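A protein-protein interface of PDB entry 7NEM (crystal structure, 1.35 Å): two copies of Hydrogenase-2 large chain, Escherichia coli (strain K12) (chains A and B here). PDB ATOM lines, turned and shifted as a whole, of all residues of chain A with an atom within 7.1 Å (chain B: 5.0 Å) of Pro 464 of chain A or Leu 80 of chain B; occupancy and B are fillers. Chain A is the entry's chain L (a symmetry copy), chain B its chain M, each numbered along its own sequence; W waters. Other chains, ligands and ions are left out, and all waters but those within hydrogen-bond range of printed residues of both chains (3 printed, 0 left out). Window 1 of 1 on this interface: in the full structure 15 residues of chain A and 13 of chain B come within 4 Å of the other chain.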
ATOM      1  N   LEU A  80      31.747  -2.626  -6.396  1.00  0.00           N
ATOM      2  CA  LEU A  80      30.697  -2.816  -7.409  1.00  0.00           C
ATOM      3  C   LEU A  80      29.444  -3.492  -6.828  1.00  0.00           C
ATOM      4  O   LEU A  80      28.433  -3.547  -7.544  1.00  0.00           O
ATOM      5  CB  LEU A  80      31.273  -3.580  -8.594  1.00  0.00           C
ATOM      6  CG  LEU A  80      32.379  -2.863  -9.358  1.00  0.00           C
ATOM      7  CD1 LEU A  80      33.153  -3.845 -10.209  1.00  0.00           C
ATOM      8  CD2 LEU A  80      31.762  -1.780 -10.234  1.00  0.00           C
ATOM      9  N   PRO A 461      30.704  -8.172 -14.406  1.00  0.00           N
ATOM     10  CA  PRO A 461      30.445  -6.866 -13.823  1.00  0.00           C
ATOM     11  C   PRO A 461      29.969  -5.830 -14.849  1.00  0.00           C
ATOM     12  O   PRO A 461      30.321  -5.868 -16.008  1.00  0.00           O
ATOM     13  CB  PRO A 461      31.775  -6.389 -13.254  1.00  0.00           C
ATOM     14  CG  PRO A 461      32.800  -7.214 -13.924  1.00  0.00           C
ATOM     15  CD  PRO A 461      32.148  -8.462 -14.452  1.00  0.00           C
ATOM     16  N   ASN A 462      29.216  -4.880 -14.335  1.00  0.00           N
ATOM     17  CA  ASN A 462      29.020  -3.585 -15.001  1.00  0.00           C
ATOM     18  C   ASN A 462      29.651  -2.527 -14.098  1.00  0.00           C
ATOM     19  O   ASN A 462      29.602  -2.612 -12.853  1.00  0.00           O
ATOM     20  CB  ASN A 462      27.546  -3.335 -15.338  1.00  0.00           C
ATOM     21  CG  ASN A 462      26.638  -3.405 -14.140  1.00  0.00           C
ATOM     22  OD1 ASN A 462      26.109  -4.467 -13.791  1.00  0.00           O
ATOM     23  ND2 ASN A 462      26.450  -2.279 -13.485  1.00  0.00           N
ATOM     24  N   ILE A 463      30.282  -1.568 -14.746  1.00  0.00           N
ATOM     25  CA  ILE A 463      31.020  -0.488 -14.046  1.00  0.00           C
ATOM     26  C   ILE A 463      30.443   0.841 -14.533  1.00  0.00           C
ATOM     27  O   ILE A 463      30.697   1.203 -15.667  1.00  0.00           O
ATOM     28  CB  ILE A 463      32.541  -0.583 -14.292  1.00  0.00           C
ATOM     29  CG1 ILE A 463      33.038  -1.990 -13.920  1.00  0.00           C
ATOM     30  CG2 ILE A 463      33.211   0.494 -13.472  1.00  0.00           C
ATOM     31  CD1 ILE A 463      34.545  -2.190 -14.053  1.00  0.00           C
ATOM     32  N   PRO A 464      29.640   1.523 -13.695  1.00  0.00           N
ATOM     33  CA  PRO A 464      29.065   2.808 -14.086  1.00  0.00           C
ATOM     34  C   PRO A 464      30.160   3.737 -14.596  1.00  0.00           C
ATOM     35  O   PRO A 464      31.249   3.768 -14.019  1.00  0.00           O
ATOM     36  CB  PRO A 464      28.399   3.316 -12.819  1.00  0.00           C
ATOM     37  CG  PRO A 464      28.017   2.064 -12.080  1.00  0.00           C
ATOM     38  CD  PRO A 464      29.184   1.133 -12.359  1.00  0.00           C
ATOM     39  N   ALA A 465      29.876   4.440 -15.695  1.00  0.00           N
ATOM     40  CA  ALA A 465      30.831   5.332 -16.371  1.00  0.00           C
ATOM     41  C   ALA A 465      30.902   6.682 -15.672  1.00  0.00           C
ATOM     42  O   ALA A 465      31.759   7.510 -16.130  1.00  0.00           O
ATOM     43  CB  ALA A 465      30.427   5.535 -17.817  1.00  0.00           C
ATOM     44  N   THR A 466      30.034   6.961 -14.721  1.00  0.00           N
ATOM     45  CA  THR A 466      29.995   8.194 -13.910  1.00  0.00           C
ATOM     46  C   THR A 466      29.839   7.773 -12.462  1.00  0.00           C
ATOM     47  O   THR A 466      29.598   6.557 -12.190  1.00  0.00           O
ATOM     48  CB  THR A 466      28.954   9.218 -14.395  1.00  0.00           C
ATOM     49  OG1 THR A 466      27.682   8.692 -14.002  1.00  0.00           O
ATOM     50  CG2 THR A 466      29.068   9.513 -15.877  1.00  0.00           C
ATOM     51  N   GLY A 467      29.997   8.718 -11.540  1.00  0.00           N
ATOM     52  CA  GLY A 467      29.930   8.442 -10.115  1.00  0.00           C
ATOM     53  C   GLY A 467      31.259   8.012  -9.535  1.00  0.00           C
ATOM     54  O   GLY A 467      32.200   7.670 -10.286  1.00  0.00           O
ATOM     55  N   PHE A 469      32.817   5.647  -6.351  1.00  0.00           N
ATOM     56  CA  PHE A 469      32.436   4.661  -5.332  1.00  0.00           C
ATOM     57  C   PHE A 469      33.663   3.855  -4.913  1.00  0.00           C
ATOM     58  O   PHE A 469      34.709   3.964  -5.559  1.00  0.00           O
ATOM     59  CB  PHE A 469      31.199   3.923  -5.819  1.00  0.00           C
ATOM     60  CG  PHE A 469      31.415   3.160  -7.086  1.00  0.00           C
ATOM     61  CD1 PHE A 469      31.400   3.778  -8.314  1.00  0.00           C
ATOM     62  CD2 PHE A 469      31.674   1.812  -7.029  1.00  0.00           C
ATOM     63  CE1 PHE A 469      31.667   3.100  -9.467  1.00  0.00           C
ATOM     64  CE2 PHE A 469      31.870   1.100  -8.200  1.00  0.00           C
ATOM     65  CZ  PHE A 469      31.877   1.740  -9.422  1.00  0.00           C
ATOM     66  N   ILE A 488      36.851   4.165  -7.379  1.00  0.00           N
ATOM     67  CA  ILE A 488      36.521   4.233  -8.822  1.00  0.00           C
ATOM     68  C   ILE A 488      35.838   5.573  -9.087  1.00  0.00           C
ATOM     69  O   ILE A 488      34.901   5.875  -8.362  1.00  0.00           O
ATOM     70  CB  ILE A 488      35.621   3.040  -9.222  1.00  0.00           C
ATOM     71  CG1 ILE A 488      36.276   1.677  -8.936  1.00  0.00           C
ATOM     72  CG2 ILE A 488      35.202   3.193 -10.676  1.00  0.00           C
ATOM     73  CD1 ILE A 488      35.361   0.508  -9.085  1.00  0.00           C
ATOM     74  N   LYS A 489      36.294   6.297 -10.091  1.00  0.00           N
ATOM     75  CA  LYS A 489      35.622   7.556 -10.489  1.00  0.00           C
ATOM     76  C   LYS A 489      35.530   7.556 -11.995  1.00  0.00           C
ATOM     77  O   LYS A 489      36.532   7.305 -12.678  1.00  0.00           O
ATOM     78  CB  LYS A 489      36.365   8.779  -9.945  1.00  0.00           C
ATOM     79  CG  LYS A 489      35.643  10.102 -10.235  1.00  0.00           C
ATOM     80  CD  LYS A 489      36.398  11.332  -9.763  1.00  0.00           C
ATOM     81  CE  LYS A 489      37.435  11.819 -10.762  1.00  0.00           C
ATOM     82  NZ  LYS A 489      38.787  11.957 -10.154  1.00  0.00           N
ATOM     83  N   ASP A 490      34.325   7.761 -12.513  1.00  0.00           N
ATOM     84  CA  ASP A 490      34.074   7.767 -13.981  1.00  0.00           C
ATOM     85  C   ASP A 490      34.679   6.526 -14.646  1.00  0.00           C
ATOM     86  O   ASP A 490      35.264   6.589 -15.740  1.00  0.00           O
ATOM     87  CB  ASP A 490      34.530   9.088 -14.597  1.00  0.00           C
ATOM     88  CG  ASP A 490      33.752  10.281 -14.046  1.00  0.00           C
ATOM     89  OD1 ASP A 490      32.702  10.100 -13.431  1.00  0.00           O
ATOM     90  OD2 ASP A 490      34.277  11.385 -14.111  1.00  0.00           O
ATOM     91  N   GLY A 491      34.544   5.416 -13.967  1.00  0.00           N
ATOM     92  CA  GLY A 491      34.784   4.077 -14.517  1.00  0.00           C
ATOM     93  C   GLY A 491      36.228   3.627 -14.390  1.00  0.00           C
ATOM     94  O   GLY A 491      36.477   2.518 -14.820  1.00  0.00           O
ATOM     95  N   ILE A 492      37.125   4.447 -13.865  1.00  0.00           N
ATOM     96  CA  ILE A 492      38.556   4.067 -13.755  1.00  0.00           C
ATOM     97  C   ILE A 492      39.011   4.229 -12.301  1.00  0.00           C
ATOM     98  O   ILE A 492      38.392   4.905 -11.485  1.00  0.00           O
ATOM     99  CB  ILE A 492      39.487   4.773 -14.779  1.00  0.00           C
ATOM    100  CG1 ILE A 492      39.553   6.271 -14.526  1.00  0.00           C
ATOM    101  CG2 ILE A 492      39.095   4.398 -16.223  1.00  0.00           C
ATOM    102  CD1 ILE A 492      40.513   6.998 -15.475  1.00  0.00           C
ATOM    103  N   ALA B  76      17.870   2.652 -16.361  1.00  0.00           N
ATOM    104  CA  ALA B  76      18.703   1.934 -15.374  1.00  0.00           C
ATOM    105  C   ALA B  76      19.963   1.407 -16.064  1.00  0.00           C
ATOM    106  O   ALA B  76      21.060   1.469 -15.488  1.00  0.00           O
ATOM    107  CB  ALA B  76      17.938   0.837 -14.706  1.00  0.00           C
ATOM    108  N   GLU B  77      19.819   0.840 -17.248  1.00  0.00           N
ATOM    109  CA  GLU B  77      20.994   0.341 -18.004  1.00  0.00           C
ATOM    110  C   GLU B  77      21.979   1.473 -18.298  1.00  0.00           C
ATOM    111  O   GLU B  77      23.201   1.228 -18.309  1.00  0.00           O
ATOM    112  CB  GLU B  77      20.489  -0.378 -19.255  1.00  0.00           C
ATOM    113  CG  GLU B  77      19.808  -1.702 -18.896  1.00  0.00           C
ATOM    114  CD  GLU B  77      18.811  -2.249 -19.915  1.00  0.00           C
ATOM    115  OE1 GLU B  77      18.536  -1.585 -20.954  1.00  0.00           O
ATOM    116  OE2 GLU B  77      18.273  -3.359 -19.622  1.00  0.00           O
ATOM    117  N   SER B  78      21.471   2.648 -18.629  1.00  0.00           N
ATOM    118  CA  SER B  78      22.296   3.856 -18.851  1.00  0.00           C
ATOM    119  C   SER B  78      23.059   4.193 -17.567  1.00  0.00           C
ATOM    120  O   SER B  78      24.338   4.372 -17.637  1.00  0.00           O
ATOM    121  CB  SER B  78      21.431   4.978 -19.295  1.00  0.00           C
ATOM    122  OG  SER B  78      22.075   6.240 -19.117  1.00  0.00           O
ATOM    123  N   ALA B  79      22.370   4.286 -16.459  1.00  0.00           N
ATOM    124  CA  ALA B  79      23.031   4.655 -15.194  1.00  0.00           C
ATOM    125  C   ALA B  79      24.125   3.633 -14.843  1.00  0.00           C
ATOM    126  O   ALA B  79      25.202   4.040 -14.386  1.00  0.00           O
ATOM    127  CB  ALA B  79      22.036   4.699 -14.080  1.00  0.00           C
ATOM    128  N   LEU B  80      23.859   2.359 -15.091  1.00  0.00           N
ATOM    129  CA  LEU B  80      24.699   1.236 -14.611  1.00  0.00           C
ATOM    130  C   LEU B  80      25.780   0.850 -15.640  1.00  0.00           C
ATOM    131  O   LEU B  80      26.667   0.077 -15.290  1.00  0.00           O
ATOM    132  CB  LEU B  80      23.838   0.036 -14.235  1.00  0.00           C
ATOM    133  CG  LEU B  80      22.901   0.272 -13.050  1.00  0.00           C
ATOM    134  CD1 LEU B  80      21.896  -0.839 -12.938  1.00  0.00           C
ATOM    135  CD2 LEU B  80      23.721   0.452 -11.764  1.00  0.00           C
ATOM    136  N   ASN B  81      25.703   1.359 -16.854  1.00  0.00           N
ATOM    137  CA  ASN B  81      26.626   1.061 -17.985  1.00  0.00           C
ATOM    138  C   ASN B  81      26.504  -0.420 -18.386  1.00  0.00           C
ATOM    139  O   ASN B  81      27.524  -1.147 -18.509  1.00  0.00           O
ATOM    140  CB  ASN B  81      28.046   1.518 -17.666  1.00  0.00           C
ATOM    141  CG  ASN B  81      28.953   1.424 -18.867  1.00  0.00           C
ATOM    142  OD1 ASN B  81      28.520   1.513 -20.010  1.00  0.00           O
ATOM    143  ND2 ASN B  81      30.240   1.286 -18.636  1.00  0.00           N
ATOM    144  N   ILE B  82      25.278  -0.864 -18.633  1.00  0.00           N
ATOM    145  CA  ILE B  82      24.996  -2.239 -19.101  1.00  0.00           C
ATOM    146  C   ILE B  82      24.736  -2.214 -20.601  1.00  0.00           C
ATOM    147  O   ILE B  82      23.895  -1.429 -21.069  1.00  0.00           O
ATOM    148  CB  ILE B  82      23.804  -2.813 -18.331  1.00  0.00           C
ATOM    149  CG1 ILE B  82      24.170  -3.016 -16.853  1.00  0.00           C
ATOM    150  CG2 ILE B  82      23.352  -4.099 -19.022  1.00  0.00           C
ATOM    151  CD1 ILE B  82      23.001  -3.229 -15.977  1.00  0.00           C
ATOM    152  N   VAL B 220      16.117  -5.020 -16.118  1.00  0.00           N
ATOM    153  CA  VAL B 220      17.397  -4.282 -16.215  1.00  0.00           C
ATOM    154  C   VAL B 220      18.477  -5.313 -16.523  1.00  0.00           C
ATOM    155  O   VAL B 220      18.753  -6.160 -15.640  1.00  0.00           O
ATOM    156  CB  VAL B 220      17.639  -3.503 -14.913  1.00  0.00           C
ATOM    157  CG1 VAL B 220      19.016  -2.858 -14.932  1.00  0.00           C
ATOM    158  CG2 VAL B 220      16.558  -2.449 -14.692  1.00  0.00           C
ATOM    159  N   PRO B 461      22.650  -7.395 -13.486  1.00  0.00           N
ATOM    160  CA  PRO B 461      23.272  -6.173 -13.006  1.00  0.00           C
ATOM    161  C   PRO B 461      23.889  -6.268 -11.618  1.00  0.00           C
ATOM    162  O   PRO B 461      23.430  -7.053 -10.798  1.00  0.00           O
ATOM    163  CB  PRO B 461      22.136  -5.140 -13.026  1.00  0.00           C
ATOM    164  CG  PRO B 461      20.884  -5.900 -13.015  1.00  0.00           C
ATOM    165  CD  PRO B 461      21.184  -7.271 -13.579  1.00  0.00           C
ATOM    166  N   ASN B 462      24.912  -5.445 -11.425  1.00  0.00           N
ATOM    167  CA  ASN B 462      25.367  -5.092 -10.072  1.00  0.00           C
ATOM    168  C   ASN B 462      25.110  -3.610  -9.863  1.00  0.00           C
ATOM    169  O   ASN B 462      25.219  -2.821 -10.803  1.00  0.00           O
ATOM    170  CB  ASN B 462      26.807  -5.521  -9.783  1.00  0.00           C
ATOM    171  CG  ASN B 462      27.797  -4.962 -10.756  1.00  0.00           C
ATOM    172  OD1 ASN B 462      28.060  -5.598 -11.768  1.00  0.00           O
ATOM    173  ND2 ASN B 462      28.278  -3.762 -10.500  1.00  0.00           N
ATOM    174  N   ILE B 463      24.662  -3.273  -8.678  1.00  0.00           N
ATOM    175  CA  ILE B 463      24.346  -1.868  -8.324  1.00  0.00           C
ATOM    176  C   ILE B 463      25.184  -1.460  -7.108  1.00  0.00           C
ATOM    177  O   ILE B 463      24.935  -1.956  -6.014  1.00  0.00           O
ATOM    178  CB  ILE B 463      22.861  -1.720  -8.016  1.00  0.00           C
ATOM    179  CG1 ILE B 463      22.048  -2.289  -9.188  1.00  0.00           C
ATOM    180  CG2 ILE B 463      22.585  -0.266  -7.696  1.00  0.00           C
ATOM    181  CD1 ILE B 463      20.548  -2.277  -8.996  1.00  0.00           C
ATOM    182  N   PRO B 464      26.214  -0.623  -7.292  1.00  0.00           N
ATOM    183  CA  PRO B 464      27.055  -0.195  -6.157  1.00  0.00           C
ATOM    184  C   PRO B 464      26.203   0.391  -5.042  1.00  0.00           C
ATOM    185  O   PRO B 464      25.234   1.080  -5.341  1.00  0.00           O
ATOM    186  CB  PRO B 464      28.031   0.802  -6.764  1.00  0.00           C
ATOM    187  CG  PRO B 464      28.104   0.435  -8.244  1.00  0.00           C
ATOM    188  CD  PRO B 464      26.697  -0.056  -8.558  1.00  0.00           C
ATOM    189  N   PHE B 469      24.778   7.849  -9.428  1.00  0.00           N
ATOM    190  CA  PHE B 469      24.843   7.406 -10.837  1.00  0.00           C
ATOM    191  C   PHE B 469      23.615   7.971 -11.495  1.00  0.00           C
ATOM    192  O   PHE B 469      22.500   7.752 -10.985  1.00  0.00           O
ATOM    193  CB  PHE B 469      24.833   5.871 -11.028  1.00  0.00           C
ATOM    194  CG  PHE B 469      25.874   5.240 -10.158  1.00  0.00           C
ATOM    195  CD1 PHE B 469      27.211   5.419 -10.504  1.00  0.00           C
ATOM    196  CD2 PHE B 469      25.566   4.469  -9.051  1.00  0.00           C
ATOM    197  CE1 PHE B 469      28.245   4.879  -9.739  1.00  0.00           C
ATOM    198  CE2 PHE B 469      26.609   3.955  -8.277  1.00  0.00           C
ATOM    199  CZ  PHE B 469      27.953   4.141  -8.639  1.00  0.00           C
ATOM    200  N   ILE B 488      20.479   7.274  -9.158  1.00  0.00           N
ATOM    201  CA  ILE B 488      20.718   6.228  -8.147  1.00  0.00           C
ATOM    202  C   ILE B 488      21.675   6.794  -7.103  1.00  0.00           C
ATOM    203  O   ILE B 488      22.721   7.299  -7.481  1.00  0.00           O
ATOM    204  CB  ILE B 488      21.246   4.931  -8.762  1.00  0.00           C
ATOM    205  CG1 ILE B 488      20.329   4.366  -9.845  1.00  0.00           C
ATOM    206  CG2 ILE B 488      21.504   3.928  -7.658  1.00  0.00           C
ATOM    207  CD1 ILE B 488      20.909   3.246 -10.620  1.00  0.00           C
HETATM  208  O   HOH W   1      30.159  -1.843 -17.536  1.00  0.00           O
HETATM  209  O   HOH W   2      27.214   4.754 -16.527  1.00  0.00           O
HETATM  210  O   HOH W   3      32.896   2.307 -16.937  1.00  0.00           O
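Pro 464 of chain A touches just these residues of chain B: Ala 79 (3.6 Å), Leu 80 (3.7 Å), Asn 81 (3.9 Å) and Phe 469 (3.3 Å).
Leu 80 of chain B touches three residues of chain A.
Printed residues of chain B within 4 Å of Ile 463 of chain A: Leu 80 (3.9 Å) and Asn 81 (3.0 Å).
Printed residues of chain A within 4 Å of Asn 81 of chain B: Asn 462, Ile 463, Pro 464 and Ala 465.
Printed residues of chain A within 4 Å of Pro 464 of chain B: Leu 80 and Phe 469.
Of the printed residues of chain B, Leu 80 of chain A touches Asn 462, Ile 463 and Pro 464.
Printed residues of chain B within 4 Å of Phe 469 of chain A: Pro 464 (3.8 Å) and Phe 469 (3.5 Å).
The backbone carbonyl oxygen (O) of Leu 80 of chain A is in hydrogen-bond range of the side-chain amide nitrogen (ND2) of Asn 462 of chain B.
The backbone NH (N) of Asn 462 of chain B sits at hydrogen-bond distance from the side-chain amide oxygen (OD1) of Asn 462 of chain A (2.8 Å).
The side-chain amide nitrogen (ND2) of Asn 81 of chain B is in hydrogen-bond range of the backbone carbonyl oxygen (O) of Ile 463 of chain A (3.0 Å).
The backbone carbonyl oxygen of Leu 80 of chain B is in hydrogen-bond range of the side-chain amide nitrogen of Asn 462 of chain A (3.0 Å).
Printed residues of chain B that touch a printed residue of chain A: Ala 79, Leu 80, Asn 81, Ile 82, Pro 461, Asn 462, Ile 463, Pro 464 and Phe 469.
Hydrophobic or aromatic side chains of chain B within 4 Å of the printed part of chain A: Leu 80, Ile 82, Pro 464 and Phe 469.
Of the 14 printed residues of chain A, 9 touch a printed residue of chain B.
Hydrophobic or aromatic side chains of chain A that line the printed part of chain B: Leu 80, Pro 464 and Phe 469.
Among the printed residues, 20 pairs touch across the chains.
N of Pro 464 of chain B touches O of Leu 80 of chain A, at 3.7 Å.
OD1 of Asn 462 of chain B touches CA of Pro 461 of chain A, at 3.4 Å.
Asn 81 of chain B touches Asn 462 of chain A (O to CB, 3.9 Å).
Pro 461 of chain B touches Asn 462 of chain A.
Leu 80 of chain B touches Ile 463 of chain A (O to C, 3.9 Å).
Pro 464 of chain A touches Asn 81 of chain B (CA to CB, 3.9 Å).
Pro 464 of chain A touches Phe 469 of chain B.
Gly 467 of chain A touches Phe 469 of chain B (CA to CE1, 3.96 Å).
CD2 of Phe 469 of chain A touches CB of Pro 464 of chain B, 3.8 Å away.
Phe 469 of chain A touches Phe 469 of chain B.
Water W3 lies within hydrogen-bond range of the backbone carbonyl oxygen of Ile 463 of chain A (2.8 Å) and the side-chain amide nitrogen of Asn 81 of chain B (3.3 Å).
Water W1 lies within hydrogen-bond range of the backbone NH of Ile 463 of chain A and the backbone carbonyl oxygen of Asn 81 of chain B.
Water W2 lies within hydrogen-bond range of the backbone NH (N) of Ala 465 of chain A (2.8 Å), the backbone carbonyl oxygen (O) of Ala 79 of chain B (3.0 Å) and the backbone carbonyl oxygen (O) of Ser 78 of chain B (3.1 Å).
O of Phe 469 of chain A sits at hydrogen-bond distance from N of Ile 488 of chain A (2.8 Å).
The backbone NH (N) of Asp 490 of chain A lies within hydrogen-bond range of the backbone carbonyl oxygen (O) of Gly 467 of chain A, at 3.1 Å.
O of Phe 469 of chain B sits at hydrogen-bond distance from N of Ile 488 of chain B (2.8 Å).
The backbone carbonyl oxygen (O) of Glu 77 of chain B sits at hydrogen-bond distance from the backbone NH (N) of Ile 82 of chain B, at 3.0 Å.
Leu 80 of chain A touches Asn 462 of chain B, and with the chains exchanged Asn 462 of chain A touches Leu 80 of chain B.
Leu 80 of chain A touches Ile 463 of chain B, and with the chains exchanged Ile 463 of chain A touches Leu 80 of chain B.
Pro 461 of chain A touches Asn 462 of chain B, and with the chains exchanged Asn 462 of chain A touches Pro 461 of chain B.
Phe 469 of chain A touches its own counterpart, Phe 469 of chain B.
Positions printed for both chains: 80, 461, 462, 463, 464, 469 and 488.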
